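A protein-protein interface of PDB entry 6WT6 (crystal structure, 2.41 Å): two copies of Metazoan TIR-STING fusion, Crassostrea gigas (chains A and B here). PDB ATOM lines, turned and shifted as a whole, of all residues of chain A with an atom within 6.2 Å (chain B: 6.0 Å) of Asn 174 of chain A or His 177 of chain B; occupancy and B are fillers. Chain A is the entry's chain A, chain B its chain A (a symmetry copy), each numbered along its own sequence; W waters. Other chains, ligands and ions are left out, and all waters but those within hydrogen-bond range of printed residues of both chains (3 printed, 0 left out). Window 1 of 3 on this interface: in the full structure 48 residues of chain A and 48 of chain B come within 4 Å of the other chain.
NE2 of His 177 of chain B sits at hydrogen-bond distance from OD1 of Asp 110 of chain A (3.4 Å).
OD1 of Asp 110 of chain A lies within salt-bridge range of NH1 of Arg 315 of chain B.
ND1 of His 177 of chain B lies within hydrogen-bond range of N of Gly 173 of chain A.
NE2 of His 177 of chain A lies within hydrogen-bond range of OD1 of Asp 110 of chain B (3.4 Å).
The side-chain carboxylate of Asp 111 of chain B sits close to the side-chain carboxylate of Asp 111 of chain A, 3.4 Å away.
The backbone NH (N) of Ser 112 of chain A is in hydrogen-bond range of the side-chain carboxylate (OD2) of Asp 110 of chain A (3.0 Å).
The backbone NH of Asn 174 of chain A lies within hydrogen-bond range of the side-chain carboxylate of Asp 111 of chain A, 2.9 Å away.
O of Gly 173 of chain A sits at hydrogen-bond distance from NE2 of Gln 305 of chain A, 2.9 Å away.
The side-chain amide oxygen (OD1) of Asn 174 of chain A sits at hydrogen-bond distance from the backbone NH (N) of Ala 176 of chain A (3.4 Å).
The side-chain amide oxygen of Asn 174 of chain A sits close to the side-chain amide oxygen of Gln 305 of chain A, 3.1 Å away.
N of Ala 176 of chain B sits at hydrogen-bond distance from OD1 of Asn 174 of chain B, at 3.4 Å.
Asn 174 of chain B touches Asp 111 of chain A (ND2 to CB, 3.2 Å).
Pro 171 of chain A touches His 177 of chain B (O to CE1, 3.8 Å).
O of Leu 175 of chain A touches CA of Gly 178 of chain B (3.7 Å).
Trp 181 of chain B touches Leu 175 of chain A (CD1 to CD2, 3.7 Å).
CD2 of His 177 of chain A touches CB of Asp 111 of chain B, at 3.5 Å.
His 177 of chain A touches Asn 174 of chain B (CB to O, 3.8 Å).
His 177 of chain A touches Leu 175 of chain B.
Gly 178 of chain A touches Leu 175 of chain B (CA to O, 3.7 Å).
Gly 178 of chain B touches Gly 178 of chain A.
Gly 182 of chain B touches Phe 179 of chain A (N to CE1, 3.9 Å).
Asn 174 of chain A touches just these residues of chain B: Asp 111 and His 177.
His 177 of chain B touches just these residues of chain A: Asp 110 (3.4 Å), Asp 111 (3.5 Å), Pro 171 (3.8 Å), Gly 173 (3.2 Å), Asn 174 (3.8 Å) and Leu 175 (3.4 Å).
Printed residues of chain B within 4 Å of Gly 178 of chain A: Leu 175 (3.7 Å), Gly 178 (3.9 Å) and Phe 179 (3.0 Å).
Printed residues of chain A within 4 Å of Phe 179 of chain B: Gly 178.
Printed residues of chain A within 4 Å of Gly 178 of chain B: Leu 175 (3.7 Å), Gly 178 (3.9 Å) and Phe 179 (3.0 Å).
Ala 176 of chain B touches none of the printed residues of chain A.
Printed residues of chain A that touch a printed residue of chain B: Asp 110, Asp 111, Pro 171, Gly 173, Asn 174, Leu 175, His 177, Gly 178, Phe 179 and Arg 308.
Along chain A the printed residues that touch a printed residue of chain B span positions 110 to 308.
Of the 16 printed residues of chain B, 11 touch a printed residue of chain A.
Printed residues of chain B that touch a printed residue of chain A: Val 109, Asp 110, Asp 111, Asn 174, Leu 175, His 177, Gly 178, Phe 179, Trp 181, Gly 182 and Arg 315.
Hydrophobic or aromatic side chains of chain B that line the printed part of chain A: Leu 175, His 177, Phe 179 and Trp 181.
Among the printed residues, Asp or Glu carboxylates within 4 Å of a Lys or Arg side-chain nitrogen of the other chain: Asp 110 of chain A with Arg 315 of chain B (3.7 Å).
Asp 111 of chain B touches its own counterpart, Asp 111 of chain A.
Asp 111 of chain A touches Asn 174 of chain B, and with the chains exchanged Asn 174 of chain A touches Asp 111 of chain B.
Leu 175 of chain A touches His 177 of chain B, and with the chains exchanged His 177 of chain A touches Leu 175 of chain B.
Gly 178 of chain B touches its own counterpart, Gly 178 of chain A.
10 positions are printed for both chains.
Of the 22 pairs that touch across the chains among the printed residues, 16 have their exchanged pair printed and touching as well.
Water W3 lies within hydrogen-bond range of OD2 of Asp 111 of chain A (2.8 Å), ND2 of Asn 174 of chain B (3.0 Å), N of His 177 of chain B (3.1 Å) and O of Asn 174 of chain A (3.4 Å).
Water W2 lies within hydrogen-bond range of OD2 of Asp 111 of chain B (2.8 Å), ND2 of Asn 174 of chain A (3.0 Å), N of His 177 of chain A (3.1 Å) and O of Asn 174 of chain B (3.4 Å).
Water W1 lies within hydrogen-bond range of O of Asn 174 of chain A, O of Asn 174 of chain B, N of Gly 178 of chain A and N of Gly 178 of chain B.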
ATOM      1  N   ASP A 110     -12.474  33.171  30.355  1.00  0.00           N
ATOM      2  CA  ASP A 110     -12.409  32.552  29.042  1.00  0.00           C
ATOM      3  C   ASP A 110     -11.854  33.532  28.014  1.00  0.00           C
ATOM      4  O   ASP A 110     -11.900  34.753  28.192  1.00  0.00           O
ATOM      5  CB  ASP A 110     -13.794  32.058  28.603  1.00  0.00           C
ATOM      6  CG  ASP A 110     -13.740  31.177  27.367  1.00  0.00           C
ATOM      7  OD1 ASP A 110     -13.208  30.051  27.462  1.00  0.00           O
ATOM      8  OD2 ASP A 110     -14.227  31.610  26.303  1.00  0.00           O
ATOM      9  N   ASP A 111     -11.326  32.967  26.924  1.00  0.00           N
ATOM     10  CA  ASP A 111     -10.753  33.775  25.852  1.00  0.00           C
ATOM     11  C   ASP A 111     -11.808  34.617  25.144  1.00  0.00           C
ATOM     12  O   ASP A 111     -11.486  35.672  24.585  1.00  0.00           O
ATOM     13  CB  ASP A 111     -10.042  32.864  24.850  1.00  0.00           C
ATOM     14  CG  ASP A 111      -9.091  33.615  23.944  1.00  0.00           C
ATOM     15  OD1 ASP A 111      -8.869  34.824  24.170  1.00  0.00           O
ATOM     16  OD2 ASP A 111      -8.562  32.991  23.002  1.00  0.00           O
ATOM     17  N   SER A 112     -13.062  34.175  25.156  1.00  0.00           N
ATOM     18  CA  SER A 112     -14.141  34.860  24.456  1.00  0.00           C
ATOM     19  C   SER A 112     -14.797  35.885  25.374  1.00  0.00           C
ATOM     20  O   SER A 112     -15.301  35.533  26.447  1.00  0.00           O
ATOM     21  CB  SER A 112     -15.174  33.849  23.961  1.00  0.00           C
ATOM     22  OG  SER A 112     -16.407  34.485  23.674  1.00  0.00           O
ATOM     23  N   PRO A 171     -19.195  29.778  21.181  1.00  0.00           N
ATOM     24  CA  PRO A 171     -18.371  30.986  21.079  1.00  0.00           C
ATOM     25  C   PRO A 171     -16.892  30.639  20.949  1.00  0.00           C
ATOM     26  O   PRO A 171     -16.374  29.858  21.748  1.00  0.00           O
ATOM     27  CB  PRO A 171     -18.658  31.726  22.395  1.00  0.00           C
ATOM     28  CG  PRO A 171     -19.544  30.796  23.222  1.00  0.00           C
ATOM     29  CD  PRO A 171     -19.476  29.445  22.584  1.00  0.00           C
ATOM     30  N   VAL A 172     -16.223  31.215  19.955  1.00  0.00           N
ATOM     31  CA  VAL A 172     -14.850  30.862  19.614  1.00  0.00           C
ATOM     32  C   VAL A 172     -13.922  31.999  20.024  1.00  0.00           C
ATOM     33  O   VAL A 172     -14.129  33.153  19.629  1.00  0.00           O
ATOM     34  CB  VAL A 172     -14.711  30.561  18.112  1.00  0.00           C
ATOM     35  CG1 VAL A 172     -13.286  30.162  17.777  1.00  0.00           C
ATOM     36  CG2 VAL A 172     -15.688  29.473  17.708  1.00  0.00           C
ATOM     37  N   GLY A 173     -12.899  31.672  20.813  1.00  0.00           N
ATOM     38  CA  GLY A 173     -11.830  32.601  21.116  1.00  0.00           C
ATOM     39  C   GLY A 173     -10.767  32.583  20.032  1.00  0.00           C
ATOM     40  O   GLY A 173     -10.926  31.982  18.968  1.00  0.00           O
ATOM     41  N   ASN A 174      -9.656  33.259  20.314  1.00  0.00           N
ATOM     42  CA  ASN A 174      -8.567  33.307  19.346  1.00  0.00           C
ATOM     43  C   ASN A 174      -7.917  31.932  19.222  1.00  0.00           C
ATOM     44  O   ASN A 174      -7.569  31.301  20.224  1.00  0.00           O
ATOM     45  CB  ASN A 174      -7.530  34.359  19.744  1.00  0.00           C
ATOM     46  CG  ASN A 174      -6.564  34.689  18.608  1.00  0.00           C
ATOM     47  OD1 ASN A 174      -6.824  34.377  17.444  1.00  0.00           O
ATOM     48  ND2 ASN A 174      -5.446  35.322  18.943  1.00  0.00           N
ATOM     49  N   LEU A 175      -7.771  31.466  17.982  1.00  0.00           N
ATOM     50  CA  LEU A 175      -7.188  30.165  17.676  1.00  0.00           C
ATOM     51  C   LEU A 175      -5.706  30.238  17.332  1.00  0.00           C
ATOM     52  O   LEU A 175      -5.042  29.194  17.302  1.00  0.00           O
ATOM     53  CB  LEU A 175      -7.940  29.512  16.499  1.00  0.00           C
ATOM     54  CG  LEU A 175      -9.443  29.268  16.651  1.00  0.00           C
ATOM     55  CD1 LEU A 175     -10.095  28.979  15.305  1.00  0.00           C
ATOM     56  CD2 LEU A 175      -9.689  28.120  17.621  1.00  0.00           C
ATOM     57  N   ALA A 176      -5.174  31.443  17.097  1.00  0.00           N
ATOM     58  CA  ALA A 176      -3.834  31.588  16.531  1.00  0.00           C
ATOM     59  C   ALA A 176      -2.777  30.868  17.363  1.00  0.00           C
ATOM     60  O   ALA A 176      -2.008  30.053  16.843  1.00  0.00           O
ATOM     61  CB  ALA A 176      -3.485  33.072  16.394  1.00  0.00           C
ATOM     62  N   HIS A 177      -2.729  31.153  18.666  1.00  0.00           N
ATOM     63  CA  HIS A 177      -1.603  30.691  19.472  1.00  0.00           C
ATOM     64  C   HIS A 177      -1.635  29.183  19.677  1.00  0.00           C
ATOM     65  O   HIS A 177      -0.590  28.525  19.615  1.00  0.00           O
ATOM     66  CB  HIS A 177      -1.583  31.431  20.809  1.00  0.00           C
ATOM     67  CG  HIS A 177      -1.122  32.850  20.693  1.00  0.00           C
ATOM     68  ND1 HIS A 177       0.151  33.250  21.037  1.00  0.00           N
ATOM     69  CD2 HIS A 177      -1.755  33.956  20.235  1.00  0.00           C
ATOM     70  CE1 HIS A 177       0.276  34.546  20.813  1.00  0.00           C
ATOM     71  NE2 HIS A 177      -0.865  34.998  20.325  1.00  0.00           N
ATOM     72  N   GLY A 178      -2.816  28.617  19.919  1.00  0.00           N
ATOM     73  CA  GLY A 178      -2.907  27.172  20.045  1.00  0.00           C
ATOM     74  C   GLY A 178      -2.520  26.460  18.765  1.00  0.00           C
ATOM     75  O   GLY A 178      -1.748  25.497  18.783  1.00  0.00           O
ATOM     76  N   PHE A 179      -3.049  26.931  17.631  1.00  0.00           N
ATOM     77  CA  PHE A 179      -2.686  26.354  16.340  1.00  0.00           C
ATOM     78  C   PHE A 179      -1.191  26.484  16.082  1.00  0.00           C
ATOM     79  O   PHE A 179      -0.520  25.500  15.751  1.00  0.00           O
ATOM     80  CB  PHE A 179      -3.480  27.026  15.211  1.00  0.00           C
ATOM     81  CG  PHE A 179      -4.914  26.565  15.096  1.00  0.00           C
ATOM     82  CD1 PHE A 179      -5.403  25.540  15.890  1.00  0.00           C
ATOM     83  CD2 PHE A 179      -5.767  27.150  14.173  1.00  0.00           C
ATOM     84  CE1 PHE A 179      -6.721  25.123  15.776  1.00  0.00           C
ATOM     85  CE2 PHE A 179      -7.085  26.732  14.054  1.00  0.00           C
ATOM     86  CZ  PHE A 179      -7.560  25.718  14.856  1.00  0.00           C
ATOM     87  N   VAL A 304      -9.950  36.350   9.565  1.00  0.00           N
ATOM     88  CA  VAL A 304      -9.227  37.036  10.634  1.00  0.00           C
ATOM     89  C   VAL A 304      -8.421  36.040  11.460  1.00  0.00           C
ATOM     90  O   VAL A 304      -7.229  36.246  11.722  1.00  0.00           O
ATOM     91  CB  VAL A 304     -10.203  37.840  11.512  1.00  0.00           C
ATOM     92  CG1 VAL A 304      -9.515  38.287  12.792  1.00  0.00           C
ATOM     93  CG2 VAL A 304     -10.736  39.039  10.740  1.00  0.00           C
ATOM     94  N   GLN A 305      -9.066  34.949  11.890  1.00  0.00           N
ATOM     95  CA  GLN A 305      -8.372  33.912  12.650  1.00  0.00           C
ATOM     96  C   GLN A 305      -7.183  33.356  11.876  1.00  0.00           C
ATOM     97  O   GLN A 305      -6.104  33.147  12.445  1.00  0.00           O
ATOM     98  CB  GLN A 305      -9.338  32.782  13.009  1.00  0.00           C
ATOM     99  CG  GLN A 305     -10.463  33.173  13.962  1.00  0.00           C
ATOM    100  CD  GLN A 305     -10.093  33.022  15.423  1.00  0.00           C
ATOM    101  OE1 GLN A 305      -8.921  32.884  15.773  1.00  0.00           O
ATOM    102  NE2 GLN A 305     -11.102  33.035  16.288  1.00  0.00           N
ATOM    103  N   ARG A 308      -4.261  35.847  11.832  1.00  0.00           N
ATOM    104  CA  ARG A 308      -3.607  35.836  13.134  1.00  0.00           C
ATOM    105  C   ARG A 308      -2.742  34.594  13.290  1.00  0.00           C
ATOM    106  O   ARG A 308      -1.598  34.679  13.751  1.00  0.00           O
ATOM    107  CB  ARG A 308      -4.646  35.911  14.250  1.00  0.00           C
ATOM    108  CG  ARG A 308      -5.260  37.278  14.446  1.00  0.00           C
ATOM    109  CD  ARG A 308      -6.458  37.180  15.365  1.00  0.00           C
ATOM    110  NE  ARG A 308      -6.980  38.493  15.721  1.00  0.00           N
ATOM    111  CZ  ARG A 308      -8.107  38.685  16.397  1.00  0.00           C
ATOM    112  NH1 ARG A 308      -8.833  37.645  16.785  1.00  0.00           N
ATOM    113  NH2 ARG A 308      -8.505  39.916  16.681  1.00  0.00           N
ATOM    114  N   PHE A 309      -3.277  33.429  12.907  1.00  0.00           N
ATOM    115  CA  PHE A 309      -2.477  32.210  12.901  1.00  0.00           C
ATOM    116  C   PHE A 309      -1.250  32.373  12.014  1.00  0.00           C
ATOM    117  O   PHE A 309      -0.127  32.034  12.412  1.00  0.00           O
ATOM    118  CB  PHE A 309      -3.323  31.025  12.433  1.00  0.00           C
ATOM    119  CG  PHE A 309      -2.505  29.833  11.992  1.00  0.00           C
ATOM    120  CD1 PHE A 309      -1.826  29.051  12.924  1.00  0.00           C
ATOM    121  CD2 PHE A 309      -2.411  29.497  10.653  1.00  0.00           C
ATOM    122  CE1 PHE A 309      -1.078  27.955  12.518  1.00  0.00           C
ATOM    123  CE2 PHE A 309      -1.663  28.405  10.244  1.00  0.00           C
ATOM    124  CZ  PHE A 309      -0.992  27.634  11.179  1.00  0.00           C
ATOM    125  N   THR A 312       1.222  34.647  13.747  1.00  0.00           N
ATOM    126  CA  THR A 312       1.837  34.069  14.937  1.00  0.00           C
ATOM    127  C   THR A 312       2.843  32.986  14.567  1.00  0.00           C
ATOM    128  O   THR A 312       3.919  32.897  15.168  1.00  0.00           O
ATOM    129  CB  THR A 312       0.764  33.504  15.868  1.00  0.00           C
ATOM    130  OG1 THR A 312      -0.200  34.522  16.162  1.00  0.00           O
ATOM    131  CG2 THR A 312       1.396  33.025  17.168  1.00  0.00           C
ATOM    132  N   VAL B 109      -4.217  43.180  15.925  1.00  0.00           N
ATOM    133  CA  VAL B 109      -4.437  42.973  17.351  1.00  0.00           C
ATOM    134  C   VAL B 109      -4.088  41.534  17.703  1.00  0.00           C
ATOM    135  O   VAL B 109      -4.483  40.595  17.001  1.00  0.00           O
ATOM    136  CB  VAL B 109      -5.886  43.321  17.729  1.00  0.00           C
ATOM    137  CG1 VAL B 109      -6.129  43.067  19.211  1.00  0.00           C
ATOM    138  CG2 VAL B 109      -6.178  44.773  17.385  1.00  0.00           C
ATOM    139  N   ASP B 110      -3.334  41.360  18.785  1.00  0.00           N
ATOM    140  CA  ASP B 110      -2.825  40.063  19.197  1.00  0.00           C
ATOM    141  C   ASP B 110      -3.530  39.586  20.460  1.00  0.00           C
ATOM    142  O   ASP B 110      -4.087  40.375  21.229  1.00  0.00           O
ATOM    143  CB  ASP B 110      -1.309  40.122  19.431  1.00  0.00           C
ATOM    144  CG  ASP B 110      -0.686  38.748  19.605  1.00  0.00           C
ATOM    145  OD1 ASP B 110      -0.650  37.982  18.620  1.00  0.00           O
ATOM    146  OD2 ASP B 110      -0.234  38.434  20.725  1.00  0.00           O
ATOM    147  N   ASP B 111      -3.492  38.266  20.664  1.00  0.00           N
ATOM    148  CA  ASP B 111      -4.125  37.657  21.829  1.00  0.00           C
ATOM    149  C   ASP B 111      -3.448  38.074  23.130  1.00  0.00           C
ATOM    150  O   ASP B 111      -4.088  38.079  24.188  1.00  0.00           O
ATOM    151  CB  ASP B 111      -4.106  36.135  21.686  1.00  0.00           C
ATOM    152  CG  ASP B 111      -5.075  35.444  22.620  1.00  0.00           C
ATOM    153  OD1 ASP B 111      -5.868  36.139  23.290  1.00  0.00           O
ATOM    154  OD2 ASP B 111      -5.042  34.198  22.682  1.00  0.00           O
ATOM    155  N   ASN B 174      -3.643  32.910  24.890  1.00  0.00           N
ATOM    156  CA  ASN B 174      -4.395  31.742  25.331  1.00  0.00           C
ATOM    157  C   ASN B 174      -4.300  30.634  24.286  1.00  0.00           C
ATOM    158  O   ASN B 174      -4.527  30.862  23.095  1.00  0.00           O
ATOM    159  CB  ASN B 174      -5.857  32.105  25.599  1.00  0.00           C
ATOM    160  CG  ASN B 174      -6.596  31.021  26.380  1.00  0.00           C
ATOM    161  OD1 ASN B 174      -5.979  30.141  26.983  1.00  0.00           O
ATOM    162  ND2 ASN B 174      -7.924  31.082  26.372  1.00  0.00           N
ATOM    163  N   LEU B 175      -3.946  29.433  24.741  1.00  0.00           N
ATOM    164  CA  LEU B 175      -3.787  28.263  23.884  1.00  0.00           C
ATOM    165  C   LEU B 175      -5.026  27.377  23.845  1.00  0.00           C
ATOM    166  O   LEU B 175      -5.114  26.503  22.973  1.00  0.00           O
ATOM    167  CB  LEU B 175      -2.586  27.420  24.357  1.00  0.00           C
ATOM    168  CG  LEU B 175      -1.211  28.089  24.405  1.00  0.00           C
ATOM    169  CD1 LEU B 175      -0.226  27.269  25.229  1.00  0.00           C
ATOM    170  CD2 LEU B 175      -0.682  28.295  22.992  1.00  0.00           C
ATOM    171  N   ALA B 176      -5.984  27.596  24.751  1.00  0.00           N
ATOM    172  CA  ALA B 176      -7.086  26.653  24.942  1.00  0.00           C
ATOM    173  C   ALA B 176      -7.846  26.389  23.646  1.00  0.00           C
ATOM    174  O   ALA B 176      -8.025  25.236  23.240  1.00  0.00           O
ATOM    175  CB  ALA B 176      -8.036  27.174  26.023  1.00  0.00           C
ATOM    176  N   HIS B 177      -8.299  27.452  22.977  1.00  0.00           N
ATOM    177  CA  HIS B 177      -9.233  27.273  21.870  1.00  0.00           C
ATOM    178  C   HIS B 177      -8.559  26.643  20.659  1.00  0.00           C
ATOM    179  O   HIS B 177      -9.147  25.775  20.002  1.00  0.00           O
ATOM    180  CB  HIS B 177      -9.877  28.611  21.511  1.00  0.00           C
ATOM    181  CG  HIS B 177     -10.898  29.062  22.507  1.00  0.00           C
ATOM    182  ND1 HIS B 177     -12.255  28.936  22.293  1.00  0.00           N
ATOM    183  CD2 HIS B 177     -10.760  29.603  23.741  1.00  0.00           C
ATOM    184  CE1 HIS B 177     -12.907  29.399  23.344  1.00  0.00           C
ATOM    185  NE2 HIS B 177     -12.024  29.808  24.237  1.00  0.00           N
ATOM    186  N   GLY B 178      -7.333  27.060  20.346  1.00  0.00           N
ATOM    187  CA  GLY B 178      -6.621  26.434  19.245  1.00  0.00           C
ATOM    188  C   GLY B 178      -6.354  24.964  19.498  1.00  0.00           C
ATOM    189  O   GLY B 178      -6.583  24.119  18.630  1.00  0.00           O
ATOM    190  N   PHE B 179      -5.868  24.640  20.701  1.00  0.00           N
ATOM    191  CA  PHE B 179      -5.639  23.244  21.064  1.00  0.00           C
ATOM    192  C   PHE B 179      -6.933  22.443  21.006  1.00  0.00           C
ATOM    193  O   PHE B 179      -6.991  21.382  20.375  1.00  0.00           O
ATOM    194  CB  PHE B 179      -5.019  23.150  22.465  1.00  0.00           C
ATOM    195  CG  PHE B 179      -3.546  23.481  22.519  1.00  0.00           C
ATOM    196  CD1 PHE B 179      -2.826  23.737  21.363  1.00  0.00           C
ATOM    197  CD2 PHE B 179      -2.879  23.516  23.733  1.00  0.00           C
ATOM    198  CE1 PHE B 179      -1.474  24.040  21.423  1.00  0.00           C
ATOM    199  CE2 PHE B 179      -1.525  23.814  23.796  1.00  0.00           C
ATOM    200  CZ  PHE B 179      -0.824  24.075  22.640  1.00  0.00           C
ATOM    201  N   ALA B 180      -7.989  22.946  21.658  1.00  0.00           N
ATOM    202  CA  ALA B 180      -9.220  22.172  21.811  1.00  0.00           C
ATOM    203  C   ALA B 180      -9.925  21.959  20.474  1.00  0.00           C
ATOM    204  O   ALA B 180     -10.284  20.828  20.126  1.00  0.00           O
ATOM    205  CB  ALA B 180     -10.154  22.860  22.807  1.00  0.00           C
ATOM    206  N   TRP B 181     -10.144  23.033  19.713  1.00  0.00           N
ATOM    207  CA  TRP B 181     -10.820  22.882  18.423  1.00  0.00           C
ATOM    208  C   TRP B 181      -9.983  22.059  17.451  1.00  0.00           C
ATOM    209  O   TRP B 181     -10.524  21.254  16.684  1.00  0.00           O
ATOM    210  CB  TRP B 181     -11.146  24.251  17.826  1.00  0.00           C
ATOM    211  CG  TRP B 181     -12.306  24.934  18.493  1.00  0.00           C
ATOM    212  CD1 TRP B 181     -12.254  26.000  19.343  1.00  0.00           C
ATOM    213  CD2 TRP B 181     -13.691  24.587  18.371  1.00  0.00           C
ATOM    214  NE1 TRP B 181     -13.519  26.343  19.752  1.00  0.00           N
ATOM    215  CE2 TRP B 181     -14.420  25.491  19.171  1.00  0.00           C
ATOM    216  CE3 TRP B 181     -14.385  23.602  17.660  1.00  0.00           C
ATOM    217  CZ2 TRP B 181     -15.809  25.439  19.282  1.00  0.00           C
ATOM    218  CZ3 TRP B 181     -15.767  23.553  17.773  1.00  0.00           C
ATOM    219  CH2 TRP B 181     -16.463  24.467  18.576  1.00  0.00           C
ATOM    220  N   GLY B 182      -8.657  22.231  17.478  1.00  0.00           N
ATOM    221  CA  GLY B 182      -7.798  21.428  16.620  1.00  0.00           C
ATOM    222  C   GLY B 182      -7.794  19.957  16.998  1.00  0.00           C
ATOM    223  O   GLY B 182      -7.731  19.083  16.130  1.00  0.00           O
ATOM    224  N   PHE B 309      -7.628  24.764  28.543  1.00  0.00           N
ATOM    225  CA  PHE B 309      -7.759  23.753  27.499  1.00  0.00           C
ATOM    226  C   PHE B 309      -8.701  22.641  27.939  1.00  0.00           C
ATOM    227  O   PHE B 309      -9.600  22.234  27.190  1.00  0.00           O
ATOM    228  CB  PHE B 309      -6.385  23.183  27.141  1.00  0.00           C
ATOM    229  CG  PHE B 309      -6.451  21.866  26.401  1.00  0.00           C
ATOM    230  CD1 PHE B 309      -6.880  21.814  25.076  1.00  0.00           C
ATOM    231  CD2 PHE B 309      -6.090  20.686  27.026  1.00  0.00           C
ATOM    232  CE1 PHE B 309      -6.936  20.605  24.398  1.00  0.00           C
ATOM    233  CE2 PHE B 309      -6.147  19.477  26.352  1.00  0.00           C
ATOM    234  CZ  PHE B 309      -6.574  19.436  25.035  1.00  0.00           C
ATOM    235  N   THR B 312     -12.247  23.947  27.891  1.00  0.00           N
ATOM    236  CA  THR B 312     -12.770  24.216  26.556  1.00  0.00           C
ATOM    237  C   THR B 312     -13.061  22.922  25.807  1.00  0.00           C
ATOM    238  O   THR B 312     -14.079  22.814  25.113  1.00  0.00           O
ATOM    239  CB  THR B 312     -11.786  25.079  25.765  1.00  0.00           C
ATOM    240  OG1 THR B 312     -11.483  26.266  26.509  1.00  0.00           O
ATOM    241  CG2 THR B 312     -12.392  25.472  24.424  1.00  0.00           C
ATOM    242  N   ARG B 315     -16.354  21.562  27.060  1.00  0.00           N
ATOM    243  CA  ARG B 315     -17.519  22.279  26.555  1.00  0.00           C
ATOM    244  C   ARG B 315     -17.872  21.820  25.146  1.00  0.00           C
ATOM    245  O   ARG B 315     -19.052  21.649  24.815  1.00  0.00           O
ATOM    246  CB  ARG B 315     -17.267  23.788  26.564  1.00  0.00           C
ATOM    247  CG  ARG B 315     -16.929  24.375  27.920  1.00  0.00           C
ATOM    248  CD  ARG B 315     -17.747  25.622  28.183  1.00  0.00           C
ATOM    249  NE  ARG B 315     -17.203  26.429  29.270  1.00  0.00           N
ATOM    250  CZ  ARG B 315     -16.503  27.542  29.089  1.00  0.00           C
ATOM    251  NH1 ARG B 315     -16.267  27.982  27.859  1.00  0.00           N
ATOM    252  NH2 ARG B 315     -16.047  28.221  30.132  1.00  0.00           N
ATOM    253  N   ILE B 316     -16.860  21.615  24.302  1.00  0.00           N
ATOM    254  CA  ILE B 316     -17.103  21.202  22.924  1.00  0.00           C
ATOM    255  C   ILE B 316     -17.655  19.782  22.882  1.00  0.00           C
ATOM    256  O   ILE B 316     -18.633  19.502  22.179  1.00  0.00           O
ATOM    257  CB  ILE B 316     -15.811  21.329  22.100  1.00  0.00           C
ATOM    258  CG1 ILE B 316     -15.332  22.781  22.084  1.00  0.00           C
ATOM    259  CG2 ILE B 316     -16.023  20.809  20.689  1.00  0.00           C
ATOM    260  CD1 ILE B 316     -13.944  22.941  21.526  1.00  0.00           C
HETATM  261  O   HOH W   1      -5.546  29.407  20.871  1.00  0.00           O
HETATM  262  O   HOH W   2      -4.719  32.798  20.299  1.00  0.00           O
HETATM  263  O   HOH W   3      -7.687  30.398  23.505  1.00  0.00           O
